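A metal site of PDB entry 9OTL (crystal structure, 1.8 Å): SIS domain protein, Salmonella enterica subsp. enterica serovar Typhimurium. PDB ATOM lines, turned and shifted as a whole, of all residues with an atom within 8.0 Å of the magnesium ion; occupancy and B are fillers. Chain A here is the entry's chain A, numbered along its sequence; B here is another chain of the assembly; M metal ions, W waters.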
ATOM      1  N   ILE A 243       7.374  21.599  -7.151  1.00  0.00           N
ATOM      2  CA  ILE A 243       7.212  20.476  -6.244  1.00  0.00           C
ATOM      3  C   ILE A 243       5.912  20.652  -5.467  1.00  0.00           C
ATOM      4  O   ILE A 243       5.691  21.700  -4.843  1.00  0.00           O
ATOM      5  CB  ILE A 243       8.450  20.401  -5.343  1.00  0.00           C
ATOM      6  CG1 ILE A 243       9.720  20.342  -6.191  1.00  0.00           C
ATOM      7  CG2 ILE A 243       8.361  19.230  -4.369  1.00  0.00           C
ATOM      8  CD1 ILE A 243      10.972  20.609  -5.402  1.00  0.00           C
ATOM      9  N   HIS A 244       5.045  19.616  -5.464  1.00  0.00           N
ATOM     10  CA  HIS A 244       3.949  19.596  -4.509  1.00  0.00           C
ATOM     11  C   HIS A 244       4.498  19.382  -3.090  1.00  0.00           C
ATOM     12  O   HIS A 244       5.222  18.398  -2.822  1.00  0.00           O
ATOM     13  CB  HIS A 244       2.927  18.536  -4.881  1.00  0.00           C
ATOM     14  CG  HIS A 244       2.039  18.842  -6.056  1.00  0.00           C
ATOM     15  ND1 HIS A 244       0.818  19.459  -5.892  1.00  0.00           N
ATOM     16  CD2 HIS A 244       2.121  18.527  -7.369  1.00  0.00           C
ATOM     17  CE1 HIS A 244       0.215  19.542  -7.080  1.00  0.00           C
ATOM     18  NE2 HIS A 244       0.970  18.962  -7.970  1.00  0.00           N
ATOM     19  N   SER A 245       4.017  20.218  -2.135  1.00  0.00           N
ATOM     20  CA  SER A 245       4.540  20.189  -0.770  1.00  0.00           C
ATOM     21  C   SER A 245       4.501  18.779  -0.180  1.00  0.00           C
ATOM     22  O   SER A 245       5.417  18.363   0.513  1.00  0.00           O
ATOM     23  CB  SER A 245       3.780  21.130   0.134  1.00  0.00           C
ATOM     24  OG  SER A 245       3.690  22.413  -0.496  1.00  0.00           O
ATOM     25  N   GLY A 246       3.404  18.083  -0.439  1.00  0.00           N
ATOM     26  CA  GLY A 246       3.187  16.795   0.175  1.00  0.00           C
ATOM     27  C   GLY A 246       4.058  15.680  -0.417  1.00  0.00           C
ATOM     28  O   GLY A 246       3.989  14.585   0.096  1.00  0.00           O
ATOM     29  N   GLU A 247       4.931  15.963  -1.418  1.00  0.00           N
ATOM     30  CA  GLU A 247       5.845  14.964  -1.978  1.00  0.00           C
ATOM     31  C   GLU A 247       7.206  14.986  -1.288  1.00  0.00           C
ATOM     32  O   GLU A 247       7.973  14.044  -1.481  1.00  0.00           O
ATOM     33  CB  GLU A 247       6.392  15.127  -3.391  1.00  0.00           C
ATOM     34  CG  GLU A 247       5.405  15.618  -4.444  1.00  0.00           C
ATOM     35  CD  GLU A 247       4.240  14.736  -4.859  1.00  0.00           C
ATOM     36  OE1 GLU A 247       3.604  14.128  -3.950  1.00  0.00           O
ATOM     37  OE2 GLU A 247       3.961  14.721  -6.110  1.00  0.00           O
ATOM     38  N   PHE A 248       7.524  16.045  -0.546  1.00  0.00           N
ATOM     39  CA  PHE A 248       8.648  16.014   0.386  1.00  0.00           C
ATOM     40  C   PHE A 248       8.456  15.210   1.670  1.00  0.00           C
ATOM     41  O   PHE A 248       9.207  15.366   2.621  1.00  0.00           O
ATOM     42  CB  PHE A 248       8.921  17.389   1.018  1.00  0.00           C
ATOM     43  CG  PHE A 248       9.694  18.313   0.097  1.00  0.00           C
ATOM     44  CD1 PHE A 248      11.047  18.087  -0.159  1.00  0.00           C
ATOM     45  CD2 PHE A 248       9.064  19.397  -0.494  1.00  0.00           C
ATOM     46  CE1 PHE A 248      11.757  18.896  -1.016  1.00  0.00           C
ATOM     47  CE2 PHE A 248       9.792  20.233  -1.331  1.00  0.00           C
ATOM     48  CZ  PHE A 248      11.136  19.985  -1.580  1.00  0.00           C
ATOM     49  N   PHE A 249       7.483  14.331   1.765  1.00  0.00           N
ATOM     50  CA  PHE A 249       7.421  13.533   2.982  1.00  0.00           C
ATOM     51  C   PHE A 249       7.988  12.148   2.685  1.00  0.00           C
ATOM     52  O   PHE A 249       8.184  11.344   3.595  1.00  0.00           O
ATOM     53  CB  PHE A 249       5.996  13.383   3.534  1.00  0.00           C
ATOM     54  CG  PHE A 249       5.211  14.662   3.734  1.00  0.00           C
ATOM     55  CD1 PHE A 249       5.860  15.895   3.801  1.00  0.00           C
ATOM     56  CD2 PHE A 249       3.817  14.628   3.845  1.00  0.00           C
ATOM     57  CE1 PHE A 249       5.115  17.058   3.985  1.00  0.00           C
ATOM     58  CE2 PHE A 249       3.082  15.789   4.050  1.00  0.00           C
ATOM     59  CZ  PHE A 249       3.733  16.997   4.113  1.00  0.00           C
ATOM     60  N   HIS A 250       8.189  11.880   1.391  1.00  0.00           N
ATOM     61  CA  HIS A 250       8.503  10.553   0.921  1.00  0.00           C
ATOM     62  C   HIS A 250       9.679  10.746  -0.008  1.00  0.00           C
ATOM     63  O   HIS A 250       9.645  11.663  -0.826  1.00  0.00           O
ATOM     64  CB  HIS A 250       7.224   9.956   0.343  1.00  0.00           C
ATOM     65  CG  HIS A 250       6.127   9.991   1.371  1.00  0.00           C
ATOM     66  ND1 HIS A 250       6.124   9.158   2.475  1.00  0.00           N
ATOM     67  CD2 HIS A 250       5.079  10.812   1.531  1.00  0.00           C
ATOM     68  CE1 HIS A 250       5.087   9.429   3.236  1.00  0.00           C
ATOM     69  NE2 HIS A 250       4.436  10.433   2.682  1.00  0.00           N
ATOM     70  N   GLY A 251      10.767   9.987   0.201  1.00  0.00           N
ATOM     71  CA  GLY A 251      11.992  10.172  -0.576  1.00  0.00           C
ATOM     72  C   GLY A 251      11.700   9.731  -1.997  1.00  0.00           C
ATOM     73  O   GLY A 251      10.671   9.091  -2.168  1.00  0.00           O
ATOM     74  N   PRO A 252      12.505  10.106  -3.021  1.00  0.00           N
ATOM     75  CA  PRO A 252      13.627  11.018  -2.855  1.00  0.00           C
ATOM     76  C   PRO A 252      13.245  12.489  -2.728  1.00  0.00           C
ATOM     77  O   PRO A 252      12.110  12.862  -2.906  1.00  0.00           O
ATOM     78  CB  PRO A 252      14.427  10.825  -4.117  1.00  0.00           C
ATOM     79  CG  PRO A 252      13.319  10.578  -5.119  1.00  0.00           C
ATOM     80  CD  PRO A 252      12.346   9.671  -4.420  1.00  0.00           C
ATOM     81  N   PHE A 253      14.235  13.307  -2.370  1.00  0.00           N
ATOM     82  CA  PHE A 253      14.094  14.712  -2.079  1.00  0.00           C
ATOM     83  C   PHE A 253      15.085  15.478  -2.963  1.00  0.00           C
ATOM     84  O   PHE A 253      16.197  15.014  -3.239  1.00  0.00           O
ATOM     85  CB  PHE A 253      14.390  15.046  -0.603  1.00  0.00           C
ATOM     86  CG  PHE A 253      13.790  14.107   0.429  1.00  0.00           C
ATOM     87  CD1 PHE A 253      12.412  13.901   0.505  1.00  0.00           C
ATOM     88  CD2 PHE A 253      14.619  13.441   1.339  1.00  0.00           C
ATOM     89  CE1 PHE A 253      11.876  13.046   1.461  1.00  0.00           C
ATOM     90  CE2 PHE A 253      14.088  12.565   2.275  1.00  0.00           C
ATOM     91  CZ  PHE A 253      12.716  12.347   2.321  1.00  0.00           C
ATOM     92  N   GLU A 254      14.665  16.676  -3.351  1.00  0.00           N
ATOM     93  CA  GLU A 254      15.414  17.527  -4.259  1.00  0.00           C
ATOM     94  C   GLU A 254      16.470  18.322  -3.481  1.00  0.00           C
ATOM     95  O   GLU A 254      16.474  19.528  -3.537  1.00  0.00           O
ATOM     96  CB  GLU A 254      14.482  18.513  -4.956  1.00  0.00           C
ATOM     97  CG  GLU A 254      13.655  17.851  -6.049  1.00  0.00           C
ATOM     98  CD  GLU A 254      12.404  17.179  -5.555  1.00  0.00           C
ATOM     99  OE1 GLU A 254      12.083  17.226  -4.331  1.00  0.00           O
ATOM    100  OE2 GLU A 254      11.706  16.706  -6.467  1.00  0.00           O
ATOM    101  N   PHE A 281      10.948  20.749   7.116  1.00  0.00           N
ATOM    102  CA  PHE A 281      11.897  19.814   6.526  1.00  0.00           C
ATOM    103  C   PHE A 281      13.042  20.529   5.802  1.00  0.00           C
ATOM    104  O   PHE A 281      14.194  20.231   6.037  1.00  0.00           O
ATOM    105  CB  PHE A 281      11.066  18.972   5.565  1.00  0.00           C
ATOM    106  CG  PHE A 281      11.834  17.837   4.913  1.00  0.00           C
ATOM    107  CD1 PHE A 281      11.976  16.627   5.565  1.00  0.00           C
ATOM    108  CD2 PHE A 281      12.424  17.996   3.675  1.00  0.00           C
ATOM    109  CE1 PHE A 281      12.680  15.583   4.979  1.00  0.00           C
ATOM    110  CE2 PHE A 281      13.142  16.952   3.092  1.00  0.00           C
ATOM    111  CZ  PHE A 281      13.255  15.749   3.745  1.00  0.00           C
ATOM    112  N   GLY B  50       4.055   8.627  -3.187  1.00  0.00           N
ATOM    113  CA  GLY B  50       5.182   8.180  -3.993  1.00  0.00           C
ATOM    114  C   GLY B  50       4.773   7.507  -5.295  1.00  0.00           C
ATOM    115  O   GLY B  50       3.975   8.038  -6.071  1.00  0.00           O
ATOM    116  N   TYR B 225       6.469  10.490 -15.279  1.00  0.00           N
ATOM    117  CA  TYR B 225       6.755  11.189 -14.046  1.00  0.00           C
ATOM    118  C   TYR B 225       7.674  10.330 -13.147  1.00  0.00           C
ATOM    119  O   TYR B 225       8.656  10.804 -12.559  1.00  0.00           O
ATOM    120  CB  TYR B 225       5.376  11.607 -13.528  1.00  0.00           C
ATOM    121  CG  TYR B 225       5.580  12.388 -12.251  1.00  0.00           C
ATOM    122  CD1 TYR B 225       6.173  13.631 -12.296  1.00  0.00           C
ATOM    123  CD2 TYR B 225       5.326  11.829 -11.019  1.00  0.00           C
ATOM    124  CE1 TYR B 225       6.440  14.338 -11.149  1.00  0.00           C
ATOM    125  CE2 TYR B 225       5.546  12.541  -9.857  1.00  0.00           C
ATOM    126  CZ  TYR B 225       6.109  13.791  -9.930  1.00  0.00           C
ATOM    127  OH  TYR B 225       6.369  14.520  -8.823  1.00  0.00           O
ATOM    128  N   ILE B 229      11.684  10.901 -11.877  1.00  0.00           N
ATOM    129  CA  ILE B 229      12.262  10.807 -10.565  1.00  0.00           C
ATOM    130  C   ILE B 229      13.335   9.688 -10.521  1.00  0.00           C
ATOM    131  O   ILE B 229      14.324   9.889  -9.819  1.00  0.00           O
ATOM    132  CB  ILE B 229      11.226  10.793  -9.412  1.00  0.00           C
ATOM    133  CG1 ILE B 229      11.068   9.501  -8.840  1.00  0.00           C
ATOM    134  CG2 ILE B 229       9.869  11.472  -9.683  1.00  0.00           C
ATOM    135  CD1 ILE B 229      11.993   9.333  -7.672  1.00  0.00           C
ATOM    136  N   PHE B 232      16.497  11.295 -11.782  1.00  0.00           N
ATOM    137  CA  PHE B 232      16.971  12.216 -10.774  1.00  0.00           C
ATOM    138  C   PHE B 232      17.744  11.420  -9.722  1.00  0.00           C
ATOM    139  O   PHE B 232      18.821  11.874  -9.284  1.00  0.00           O
ATOM    140  CB  PHE B 232      15.813  13.075 -10.220  1.00  0.00           C
ATOM    141  CG  PHE B 232      16.325  13.864  -9.035  1.00  0.00           C
ATOM    142  CD1 PHE B 232      17.195  14.933  -9.234  1.00  0.00           C
ATOM    143  CD2 PHE B 232      16.059  13.462  -7.751  1.00  0.00           C
ATOM    144  CE1 PHE B 232      17.735  15.602  -8.151  1.00  0.00           C
ATOM    145  CE2 PHE B 232      16.578  14.177  -6.676  1.00  0.00           C
ATOM    146  CZ  PHE B 232      17.422  15.222  -6.885  1.00  0.00           C
ATOM    147  N   HIS B 239      16.316  18.148 -10.195  1.00  0.00           N
ATOM    148  CA  HIS B 239      15.106  17.473 -10.646  1.00  0.00           C
ATOM    149  C   HIS B 239      14.396  18.340 -11.686  1.00  0.00           C
ATOM    150  O   HIS B 239      13.915  19.412 -11.379  1.00  0.00           O
ATOM    151  CB  HIS B 239      14.190  17.101  -9.501  1.00  0.00           C
ATOM    152  CG  HIS B 239      13.021  16.309  -9.938  1.00  0.00           C
ATOM    153  ND1 HIS B 239      11.866  16.193  -9.189  1.00  0.00           N
ATOM    154  CD2 HIS B 239      12.858  15.556 -11.059  1.00  0.00           C
ATOM    155  CE1 HIS B 239      11.025  15.401  -9.852  1.00  0.00           C
ATOM    156  NE2 HIS B 239      11.604  14.994 -10.978  1.00  0.00           N
ATOM    157  N   TRP B 341      17.779   7.118  -0.581  1.00  0.00           N
ATOM    158  CA  TRP B 341      16.476   7.422   0.001  1.00  0.00           C
ATOM    159  C   TRP B 341      15.726   6.128   0.214  1.00  0.00           C
ATOM    160  O   TRP B 341      15.961   5.184  -0.517  1.00  0.00           O
ATOM    161  CB  TRP B 341      15.671   8.312  -0.966  1.00  0.00           C
ATOM    162  CG  TRP B 341      16.300   9.634  -1.265  1.00  0.00           C
ATOM    163  CD1 TRP B 341      16.222  10.764  -0.491  1.00  0.00           C
ATOM    164  CD2 TRP B 341      17.101   9.986  -2.412  1.00  0.00           C
ATOM    165  NE1 TRP B 341      16.879  11.782  -1.094  1.00  0.00           N
ATOM    166  CE2 TRP B 341      17.439  11.349  -2.269  1.00  0.00           C
ATOM    167  CE3 TRP B 341      17.547   9.299  -3.549  1.00  0.00           C
ATOM    168  CZ2 TRP B 341      18.202  12.035  -3.206  1.00  0.00           C
ATOM    169  CZ3 TRP B 341      18.307   9.983  -4.468  1.00  0.00           C
ATOM    170  CH2 TRP B 341      18.606  11.331  -4.318  1.00  0.00           C
ATOM    171  N   LYS B 342      14.771   6.129   1.147  1.00  0.00           N
ATOM    172  CA  LYS B 342      13.725   5.123   1.214  1.00  0.00           C
ATOM    173  C   LYS B 342      12.619   5.571   0.255  1.00  0.00           C
ATOM    174  O   LYS B 342      11.952   6.564   0.518  1.00  0.00           O
ATOM    175  CB  LYS B 342      13.229   5.006   2.662  1.00  0.00           C
ATOM    176  CG  LYS B 342      12.165   3.949   2.926  1.00  0.00           C
ATOM    177  CD  LYS B 342      10.984   4.436   3.781  1.00  0.00           C
ATOM    178  CE  LYS B 342      11.195   4.444   5.261  1.00  0.00           C
ATOM    179  NZ  LYS B 342      12.440   5.118   5.648  1.00  0.00           N
ATOM    180  N   GLU B 344       9.198   4.920  -2.029  1.00  0.00           N
ATOM    181  CA  GLU B 344       7.939   4.249  -1.775  1.00  0.00           C
ATOM    182  C   GLU B 344       7.459   3.624  -3.083  1.00  0.00           C
ATOM    183  O   GLU B 344       7.137   4.360  -4.006  1.00  0.00           O
ATOM    184  CB  GLU B 344       6.979   5.286  -1.206  1.00  0.00           C
ATOM    185  CG  GLU B 344       6.176   4.791  -0.010  1.00  0.00           C
ATOM    186  CD  GLU B 344       5.898   5.918   0.961  1.00  0.00           C
ATOM    187  OE1 GLU B 344       6.244   7.068   0.608  1.00  0.00           O
ATOM    188  OE2 GLU B 344       5.360   5.653   2.056  1.00  0.00           O
HETATM  189 MG    MG M   1       9.929  13.394  -2.383  1.00  0.00          MG
HETATM  190  O   HOH W   1       8.956  13.083  -4.291  1.00  0.00           O
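ND1 of His 250 is in hydrogen-bond range of OE1 of Glu 344 of chain B, at 2.8 Å.
Residues that only touch the magnesium ion: Phe 253 (3.8 Å). Of the 21 residues printed, 4 come within 4 Å of the magnesium ion. Along chain A the residues within 4 Å of the magnesium ion span positions 247 to 253.
Water W1 is bound to the magnesium ion (2.2 Å). The backbone carbonyl oxygen (O) of Glu 247 binds the magnesium ion (2.2 Å). The backbone carbonyl oxygen (O) of Pro 252 binds the magnesium ion, at 2.3 Å. The backbone carbonyl oxygen (O) of His 250 binds the magnesium ion (2.3 Å).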
